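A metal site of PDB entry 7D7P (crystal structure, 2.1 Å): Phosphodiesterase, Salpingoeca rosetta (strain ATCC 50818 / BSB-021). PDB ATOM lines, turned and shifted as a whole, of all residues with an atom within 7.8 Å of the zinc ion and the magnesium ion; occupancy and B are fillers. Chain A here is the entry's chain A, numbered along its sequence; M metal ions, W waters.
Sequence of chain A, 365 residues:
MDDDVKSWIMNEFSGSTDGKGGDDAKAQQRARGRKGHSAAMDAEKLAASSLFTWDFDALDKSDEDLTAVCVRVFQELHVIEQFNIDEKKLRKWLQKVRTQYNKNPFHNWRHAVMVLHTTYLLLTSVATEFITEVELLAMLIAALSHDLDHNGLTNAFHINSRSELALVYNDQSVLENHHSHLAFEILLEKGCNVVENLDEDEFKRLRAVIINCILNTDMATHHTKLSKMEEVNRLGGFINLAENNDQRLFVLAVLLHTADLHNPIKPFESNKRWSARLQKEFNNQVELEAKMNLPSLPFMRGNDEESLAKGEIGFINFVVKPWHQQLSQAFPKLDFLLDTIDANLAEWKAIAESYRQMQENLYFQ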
ATOM      1  N   TYR A 101      -4.414  24.986  19.765  1.00  0.00           N
ATOM      2  CA  TYR A 101      -5.207  26.188  19.938  1.00  0.00           C
ATOM      3  C   TYR A 101      -4.279  27.396  19.920  1.00  0.00           C
ATOM      4  O   TYR A 101      -3.113  27.316  20.316  1.00  0.00           O
ATOM      5  CB  TYR A 101      -6.011  26.152  21.234  1.00  0.00           C
ATOM      6  CG  TYR A 101      -7.325  25.404  21.091  1.00  0.00           C
ATOM      7  CD1 TYR A 101      -7.385  24.025  21.261  1.00  0.00           C
ATOM      8  CD2 TYR A 101      -8.492  26.078  20.768  1.00  0.00           C
ATOM      9  CE1 TYR A 101      -8.574  23.343  21.112  1.00  0.00           C
ATOM     10  CE2 TYR A 101      -9.690  25.402  20.626  1.00  0.00           C
ATOM     11  CZ  TYR A 101      -9.731  24.032  20.802  1.00  0.00           C
ATOM     12  OH  TYR A 101     -10.919  23.350  20.653  1.00  0.00           O
ATOM     13  N   PHE A 106     -10.877  35.044  22.716  1.00  0.00           N
ATOM     14  CA  PHE A 106     -12.014  34.192  23.029  1.00  0.00           C
ATOM     15  C   PHE A 106     -11.791  32.751  22.595  1.00  0.00           C
ATOM     16  O   PHE A 106     -11.881  31.837  23.413  1.00  0.00           O
ATOM     17  CB  PHE A 106     -13.289  34.748  22.381  1.00  0.00           C
ATOM     18  CG  PHE A 106     -14.541  33.975  22.734  1.00  0.00           C
ATOM     19  CD1 PHE A 106     -14.884  32.813  22.046  1.00  0.00           C
ATOM     20  CD2 PHE A 106     -15.364  34.412  23.757  1.00  0.00           C
ATOM     21  CE1 PHE A 106     -16.022  32.111  22.372  1.00  0.00           C
ATOM     22  CE2 PHE A 106     -16.511  33.703  24.090  1.00  0.00           C
ATOM     23  CZ  PHE A 106     -16.835  32.556  23.401  1.00  0.00           C
ATOM     24  N   HIS A 107     -11.509  32.516  21.301  1.00  0.00           N
ATOM     25  CA  HIS A 107     -11.424  31.151  20.773  1.00  0.00           C
ATOM     26  C   HIS A 107     -10.054  30.578  21.102  1.00  0.00           C
ATOM     27  O   HIS A 107      -9.161  30.474  20.251  1.00  0.00           O
ATOM     28  CB  HIS A 107     -11.703  31.135  19.277  1.00  0.00           C
ATOM     29  CG  HIS A 107     -13.135  31.433  18.922  1.00  0.00           C
ATOM     30  ND1 HIS A 107     -13.571  32.696  18.582  1.00  0.00           N
ATOM     31  CD2 HIS A 107     -14.223  30.635  18.863  1.00  0.00           C
ATOM     32  CE1 HIS A 107     -14.866  32.654  18.329  1.00  0.00           C
ATOM     33  NE2 HIS A 107     -15.288  31.419  18.496  1.00  0.00           N
ATOM     34  N   ASN A 108      -9.882  30.205  22.367  1.00  0.00           N
ATOM     35  CA  ASN A 108      -8.606  29.734  22.876  1.00  0.00           C
ATOM     36  C   ASN A 108      -8.760  28.423  23.638  1.00  0.00           C
ATOM     37  O   ASN A 108      -9.852  27.842  23.666  1.00  0.00           O
ATOM     38  CB  ASN A 108      -7.961  30.801  23.776  1.00  0.00           C
ATOM     39  CG  ASN A 108      -8.921  31.344  24.824  1.00  0.00           C
ATOM     40  OD1 ASN A 108      -9.616  30.571  25.494  1.00  0.00           O
ATOM     41  ND2 ASN A 108      -8.960  32.656  24.978  1.00  0.00           N
ATOM     42  N   HIS A 111     -11.535  28.409  26.232  1.00  0.00           N
ATOM     43  CA  HIS A 111     -12.877  28.218  25.662  1.00  0.00           C
ATOM     44  C   HIS A 111     -13.160  26.750  25.408  1.00  0.00           C
ATOM     45  O   HIS A 111     -14.284  26.272  25.651  1.00  0.00           O
ATOM     46  CB  HIS A 111     -13.009  29.026  24.366  1.00  0.00           C
ATOM     47  CG  HIS A 111     -14.267  28.731  23.602  1.00  0.00           C
ATOM     48  ND1 HIS A 111     -15.521  28.892  24.144  1.00  0.00           N
ATOM     49  CD2 HIS A 111     -14.460  28.280  22.341  1.00  0.00           C
ATOM     50  CE1 HIS A 111     -16.437  28.558  23.249  1.00  0.00           C
ATOM     51  NE2 HIS A 111     -15.811  28.187  22.141  1.00  0.00           N
ATOM     52  N   ALA A 112     -12.164  26.007  24.931  1.00  0.00           N
ATOM     53  CA  ALA A 112     -12.339  24.570  24.709  1.00  0.00           C
ATOM     54  C   ALA A 112     -12.664  23.851  26.015  1.00  0.00           C
ATOM     55  O   ALA A 112     -13.544  22.981  26.049  1.00  0.00           O
ATOM     56  CB  ALA A 112     -11.097  23.984  24.056  1.00  0.00           C
ATOM     57  N   VAL A 115     -16.216  24.478  27.056  1.00  0.00           N
ATOM     58  CA  VAL A 115     -17.199  23.701  26.322  1.00  0.00           C
ATOM     59  C   VAL A 115     -17.159  22.244  26.749  1.00  0.00           C
ATOM     60  O   VAL A 115     -18.193  21.563  26.817  1.00  0.00           O
ATOM     61  CB  VAL A 115     -16.991  23.875  24.807  1.00  0.00           C
ATOM     62  CG1 VAL A 115     -17.925  22.970  24.008  1.00  0.00           C
ATOM     63  CG2 VAL A 115     -17.210  25.329  24.418  1.00  0.00           C
ATOM     64  N   ALA A 143     -15.978  18.113  22.101  1.00  0.00           N
ATOM     65  CA  ALA A 143     -16.084  19.393  22.796  1.00  0.00           C
ATOM     66  C   ALA A 143     -14.725  20.065  22.936  1.00  0.00           C
ATOM     67  O   ALA A 143     -14.603  21.277  22.732  1.00  0.00           O
ATOM     68  CB  ALA A 143     -16.715  19.189  24.171  1.00  0.00           C
ATOM     69  N   HIS A 146     -13.433  21.193  19.269  1.00  0.00           N
ATOM     70  CA  HIS A 146     -14.414  21.776  18.352  1.00  0.00           C
ATOM     71  C   HIS A 146     -13.947  23.088  17.713  1.00  0.00           C
ATOM     72  O   HIS A 146     -14.538  23.510  16.714  1.00  0.00           O
ATOM     73  CB  HIS A 146     -15.740  22.012  19.076  1.00  0.00           C
ATOM     74  CG  HIS A 146     -15.782  23.273  19.870  1.00  0.00           C
ATOM     75  ND1 HIS A 146     -15.206  23.403  21.108  1.00  0.00           N
ATOM     76  CD2 HIS A 146     -16.334  24.482  19.585  1.00  0.00           C
ATOM     77  CE1 HIS A 146     -15.393  24.628  21.560  1.00  0.00           C
ATOM     78  NE2 HIS A 146     -16.079  25.297  20.655  1.00  0.00           N
ATOM     79  N   ASP A 147     -12.919  23.745  18.269  1.00  0.00           N
ATOM     80  CA  ASP A 147     -12.448  25.020  17.730  1.00  0.00           C
ATOM     81  C   ASP A 147     -10.948  24.999  17.467  1.00  0.00           C
ATOM     82  O   ASP A 147     -10.297  26.037  17.562  1.00  0.00           O
ATOM     83  CB  ASP A 147     -12.800  26.168  18.678  1.00  0.00           C
ATOM     84  CG  ASP A 147     -14.091  26.871  18.284  1.00  0.00           C
ATOM     85  OD1 ASP A 147     -14.507  26.763  17.106  1.00  0.00           O
ATOM     86  OD2 ASP A 147     -14.683  27.551  19.155  1.00  0.00           O
ATOM     87  N   LEU A 148     -10.402  23.840  17.112  1.00  0.00           N
ATOM     88  CA  LEU A 148      -8.961  23.692  16.941  1.00  0.00           C
ATOM     89  C   LEU A 148      -8.428  24.644  15.867  1.00  0.00           C
ATOM     90  O   LEU A 148      -8.987  24.736  14.773  1.00  0.00           O
ATOM     91  CB  LEU A 148      -8.617  22.255  16.570  1.00  0.00           C
ATOM     92  CG  LEU A 148      -8.514  21.246  17.715  1.00  0.00           C
ATOM     93  CD1 LEU A 148      -8.666  19.835  17.165  1.00  0.00           C
ATOM     94  CD2 LEU A 148      -7.186  21.394  18.450  1.00  0.00           C
ATOM     95  N   HIS A 150      -8.453  27.802  15.614  1.00  0.00           N
ATOM     96  CA  HIS A 150      -9.167  29.043  15.358  1.00  0.00           C
ATOM     97  C   HIS A 150      -8.196  30.216  15.412  1.00  0.00           C
ATOM     98  O   HIS A 150      -7.247  30.213  16.205  1.00  0.00           O
ATOM     99  CB  HIS A 150     -10.283  29.226  16.393  1.00  0.00           C
ATOM    100  CG  HIS A 150     -11.460  30.003  15.908  1.00  0.00           C
ATOM    101  ND1 HIS A 150     -11.429  31.365  15.711  1.00  0.00           N
ATOM    102  CD2 HIS A 150     -12.721  29.606  15.603  1.00  0.00           C
ATOM    103  CE1 HIS A 150     -12.609  31.776  15.289  1.00  0.00           C
ATOM    104  NE2 HIS A 150     -13.419  30.735  15.218  1.00  0.00           N
ATOM    105  N   ASN A 155     -16.287  32.556   9.517  1.00  0.00           N
ATOM    106  CA  ASN A 155     -16.406  31.895   8.224  1.00  0.00           C
ATOM    107  C   ASN A 155     -16.598  32.885   7.096  1.00  0.00           C
ATOM    108  O   ASN A 155     -16.104  32.675   5.981  1.00  0.00           O
ATOM    109  CB  ASN A 155     -17.569  30.898   8.249  1.00  0.00           C
ATOM    110  CG  ASN A 155     -17.172  29.552   8.827  1.00  0.00           C
ATOM    111  OD1 ASN A 155     -16.022  29.130   8.705  1.00  0.00           O
ATOM    112  ND2 ASN A 155     -18.134  28.856   9.426  1.00  0.00           N
ATOM    113  N   LEU A 175     -14.547  26.697   8.760  1.00  0.00           N
ATOM    114  CA  LEU A 175     -13.809  26.533  10.004  1.00  0.00           C
ATOM    115  C   LEU A 175     -14.134  25.205  10.685  1.00  0.00           C
ATOM    116  O   LEU A 175     -13.233  24.507  11.156  1.00  0.00           O
ATOM    117  CB  LEU A 175     -14.122  27.691  10.958  1.00  0.00           C
ATOM    118  CG  LEU A 175     -13.450  29.029  10.646  1.00  0.00           C
ATOM    119  CD1 LEU A 175     -13.905  30.073  11.643  1.00  0.00           C
ATOM    120  CD2 LEU A 175     -11.945  28.874  10.666  1.00  0.00           C
ATOM    121  N   GLU A 176     -15.421  24.847  10.740  1.00  0.00           N
ATOM    122  CA  GLU A 176     -15.823  23.627  11.430  1.00  0.00           C
ATOM    123  C   GLU A 176     -15.269  22.387  10.746  1.00  0.00           C
ATOM    124  O   GLU A 176     -14.857  21.432  11.430  1.00  0.00           O
ATOM    125  CB  GLU A 176     -17.351  23.566  11.514  1.00  0.00           C
ATOM    126  CG  GLU A 176     -17.982  24.655  12.391  1.00  0.00           C
ATOM    127  CD  GLU A 176     -17.971  26.026  11.734  1.00  0.00           C
ATOM    128  OE1 GLU A 176     -17.931  26.102  10.483  1.00  0.00           O
ATOM    129  OE2 GLU A 176     -17.997  27.036  12.465  1.00  0.00           O
ATOM    130  N   HIS A 179     -11.730  22.299  11.921  1.00  0.00           N
ATOM    131  CA  HIS A 179     -11.610  21.835  13.297  1.00  0.00           C
ATOM    132  C   HIS A 179     -11.712  20.313  13.369  1.00  0.00           C
ATOM    133  O   HIS A 179     -10.891  19.646  14.009  1.00  0.00           O
ATOM    134  CB  HIS A 179     -12.680  22.474  14.171  1.00  0.00           C
ATOM    135  CG  HIS A 179     -12.686  23.977  14.144  1.00  0.00           C
ATOM    136  ND1 HIS A 179     -11.526  24.724  14.084  1.00  0.00           N
ATOM    137  CD2 HIS A 179     -13.700  24.865  14.175  1.00  0.00           C
ATOM    138  CE1 HIS A 179     -11.837  26.008  14.075  1.00  0.00           C
ATOM    139  NE2 HIS A 179     -13.148  26.123  14.124  1.00  0.00           N
ATOM    140  N   ILE A 214     -19.376  18.571  15.655  1.00  0.00           N
ATOM    141  CA  ILE A 214     -18.530  19.725  15.394  1.00  0.00           C
ATOM    142  C   ILE A 214     -19.071  20.538  14.217  1.00  0.00           C
ATOM    143  O   ILE A 214     -19.087  21.774  14.262  1.00  0.00           O
ATOM    144  CB  ILE A 214     -17.070  19.283  15.147  1.00  0.00           C
ATOM    145  CG1 ILE A 214     -16.439  18.802  16.453  1.00  0.00           C
ATOM    146  CG2 ILE A 214     -16.249  20.423  14.554  1.00  0.00           C
ATOM    147  CD1 ILE A 214     -15.021  18.277  16.297  1.00  0.00           C
ATOM    148  N   THR A 217     -21.726  22.913  15.161  1.00  0.00           N
ATOM    149  CA  THR A 217     -21.387  24.140  15.867  1.00  0.00           C
ATOM    150  C   THR A 217     -21.319  25.344  14.935  1.00  0.00           C
ATOM    151  O   THR A 217     -21.138  26.469  15.415  1.00  0.00           O
ATOM    152  CB  THR A 217     -20.059  23.998  16.611  1.00  0.00           C
ATOM    153  OG1 THR A 217     -18.990  23.797  15.685  1.00  0.00           O
ATOM    154  CG2 THR A 217     -20.117  22.827  17.598  1.00  0.00           C
ATOM    155  N   ASP A 218     -21.460  25.128  13.624  1.00  0.00           N
ATOM    156  CA  ASP A 218     -21.565  26.218  12.673  1.00  0.00           C
ATOM    157  C   ASP A 218     -22.849  27.007  12.933  1.00  0.00           C
ATOM    158  O   ASP A 218     -23.946  26.469  12.824  1.00  0.00           O
ATOM    159  CB  ASP A 218     -21.564  25.658  11.245  1.00  0.00           C
ATOM    160  CG  ASP A 218     -21.551  26.743  10.172  1.00  0.00           C
ATOM    161  OD1 ASP A 218     -21.588  27.938  10.517  1.00  0.00           O
ATOM    162  OD2 ASP A 218     -21.489  26.384   8.972  1.00  0.00           O
ATOM    163  N   MET A 219     -22.681  28.288  13.284  1.00  0.00           N
ATOM    164  CA  MET A 219     -23.837  29.131  13.595  1.00  0.00           C
ATOM    165  C   MET A 219     -24.818  29.211  12.431  1.00  0.00           C
ATOM    166  O   MET A 219     -26.013  29.450  12.649  1.00  0.00           O
ATOM    167  CB  MET A 219     -23.366  30.528  13.985  1.00  0.00           C
ATOM    168  CG  MET A 219     -22.483  30.580  15.222  1.00  0.00           C
ATOM    169  SD  MET A 219     -23.255  29.852  16.677  1.00  0.00           S
ATOM    170  CE  MET A 219     -24.802  30.759  16.715  1.00  0.00           C
ATOM    171  N   LEU A 256     -24.170  19.882  22.274  1.00  0.00           N
ATOM    172  CA  LEU A 256     -22.842  20.478  22.092  1.00  0.00           C
ATOM    173  C   LEU A 256     -22.952  21.922  21.631  1.00  0.00           C
ATOM    174  O   LEU A 256     -22.162  22.782  22.053  1.00  0.00           O
ATOM    175  CB  LEU A 256     -22.012  19.666  21.097  1.00  0.00           C
ATOM    176  CG  LEU A 256     -20.603  20.238  20.887  1.00  0.00           C
ATOM    177  CD1 LEU A 256     -19.800  20.167  22.182  1.00  0.00           C
ATOM    178  CD2 LEU A 256     -19.855  19.548  19.752  1.00  0.00           C
ATOM    179  N   ALA A 259     -23.572  23.897  24.697  1.00  0.00           N
ATOM    180  CA  ALA A 259     -22.380  24.140  25.501  1.00  0.00           C
ATOM    181  C   ALA A 259     -21.440  25.136  24.836  1.00  0.00           C
ATOM    182  O   ALA A 259     -20.715  25.857  25.528  1.00  0.00           O
ATOM    183  CB  ALA A 259     -21.640  22.822  25.768  1.00  0.00           C
ATOM    184  N   ASP A 260     -21.451  25.204  23.500  1.00  0.00           N
ATOM    185  CA  ASP A 260     -20.621  26.176  22.796  1.00  0.00           C
ATOM    186  C   ASP A 260     -21.025  27.608  23.155  1.00  0.00           C
ATOM    187  O   ASP A 260     -20.171  28.487  23.305  1.00  0.00           O
ATOM    188  CB  ASP A 260     -20.715  25.953  21.287  1.00  0.00           C
ATOM    189  CG  ASP A 260     -19.627  26.670  20.522  1.00  0.00           C
ATOM    190  OD1 ASP A 260     -18.642  27.094  21.155  1.00  0.00           O
ATOM    191  OD2 ASP A 260     -19.753  26.821  19.283  1.00  0.00           O
ATOM    192  N   LEU A 261     -22.332  27.850  23.304  1.00  0.00           N
ATOM    193  CA  LEU A 261     -22.839  29.168  23.663  1.00  0.00           C
ATOM    194  C   LEU A 261     -22.977  29.284  25.189  1.00  0.00           C
ATOM    195  O   LEU A 261     -24.063  29.484  25.726  1.00  0.00           O
ATOM    196  CB  LEU A 261     -24.165  29.433  22.961  1.00  0.00           C
ATOM    197  CG  LEU A 261     -24.193  29.263  21.441  1.00  0.00           C
ATOM    198  CD1 LEU A 261     -25.576  29.539  20.888  1.00  0.00           C
ATOM    199  CD2 LEU A 261     -23.155  30.153  20.781  1.00  0.00           C
ATOM    200  N   HIS A 262     -21.842  29.161  25.872  1.00  0.00           N
ATOM    201  CA  HIS A 262     -21.850  29.112  27.334  1.00  0.00           C
ATOM    202  C   HIS A 262     -21.904  30.492  27.981  1.00  0.00           C
ATOM    203  O   HIS A 262     -22.187  30.573  29.178  1.00  0.00           O
ATOM    204  CB  HIS A 262     -20.604  28.362  27.838  1.00  0.00           C
ATOM    205  CG  HIS A 262     -19.309  28.917  27.354  1.00  0.00           C
ATOM    206  ND1 HIS A 262     -18.804  30.127  27.789  1.00  0.00           N
ATOM    207  CD2 HIS A 262     -18.401  28.437  26.474  1.00  0.00           C
ATOM    208  CE1 HIS A 262     -17.649  30.361  27.191  1.00  0.00           C
ATOM    209  NE2 HIS A 262     -17.383  29.350  26.386  1.00  0.00           N
HETATM  210 ZN    ZN M   1     -16.605  27.378  20.194  1.00  0.00          ZN
HETATM  211 MG    MG M   2     -16.433  27.248  16.260  1.00  0.00          MG
HETATM  212  O   HOH W   1     -16.750  25.081  15.868  1.00  0.00           O
HETATM  213  O   HOH W   2     -17.224  29.620  19.668  1.00  0.00           O
HETATM  214  O   HOH W   3     -16.383  29.423  16.896  1.00  0.00           O
HETATM  215  O   HOH W   4     -15.577  27.845  14.506  1.00  0.00           O
HETATM  216  O   HOH W   5     -18.324  27.319  15.217  1.00  0.00           O
HETATM  217  O   HOH W   6     -17.561  26.932  17.939  1.00  0.00           O
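OH of Tyr 101 is in hydrogen-bond range of N of Asp 147 (3.1 Å).
OD1 of Asn 108 is in hydrogen-bond range of N of His 111, at 3.0 Å.
A ring nitrogen (ND1) of His 146 lies within hydrogen-bond range of the backbone carbonyl oxygen (O) of Ala 143, 2.7 Å away.
NE2 of His 262 lies within hydrogen-bond range of ND1 of His 111 (3.0 Å).
OD1 of Asp 147 lies close to NE2 of His 179 (3.3 Å).
Within 4 Å of the zinc ion: His 111, His 146, Asp 147 and Asp 260.
The nearest printed residue that does not touch the zinc ion is His 107 (4.2 Å).
The nearest printed residue that does not touch the magnesium ion is His 179 (4.1 Å).
OD2 of Asp 147 is bound to the zinc ion.
NE2 of His 146 is bound to the zinc ion, 2.2 Å away.
A ring nitrogen (NE2) of His 111 binds the zinc ion.
OD1 of Asp 260 binds the zinc ion (2.3 Å).
Water W2 binds the zinc ion (2.4 Å).
The zinc ion is bound by water W6 (2.5 Å).
The zinc ion has six donor atoms within binding distance.
The magnesium ion is bound by water W4 (2.0 Å), water W6 (2.0 Å), OD1 of Asp 147 (2.2 Å), water W5 (2.2 Å), water W1 (2.2 Å) and water W3 (2.3 Å).
Water W4 lies within hydrogen-bond range of NE2 of His 179 (3.0 Å) and OE2 of Glu 176 (3.3 Å).
Water W5 lies within hydrogen-bond range of the side-chain carboxylate (OE2) of Glu 176 (2.8 Å) and the backbone carbonyl oxygen (O) of Thr 217 (2.9 Å).
Water W1 lies within hydrogen-bond range of OG1 of Thr 217 (2.6 Å) and O of His 146 (2.8 Å).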
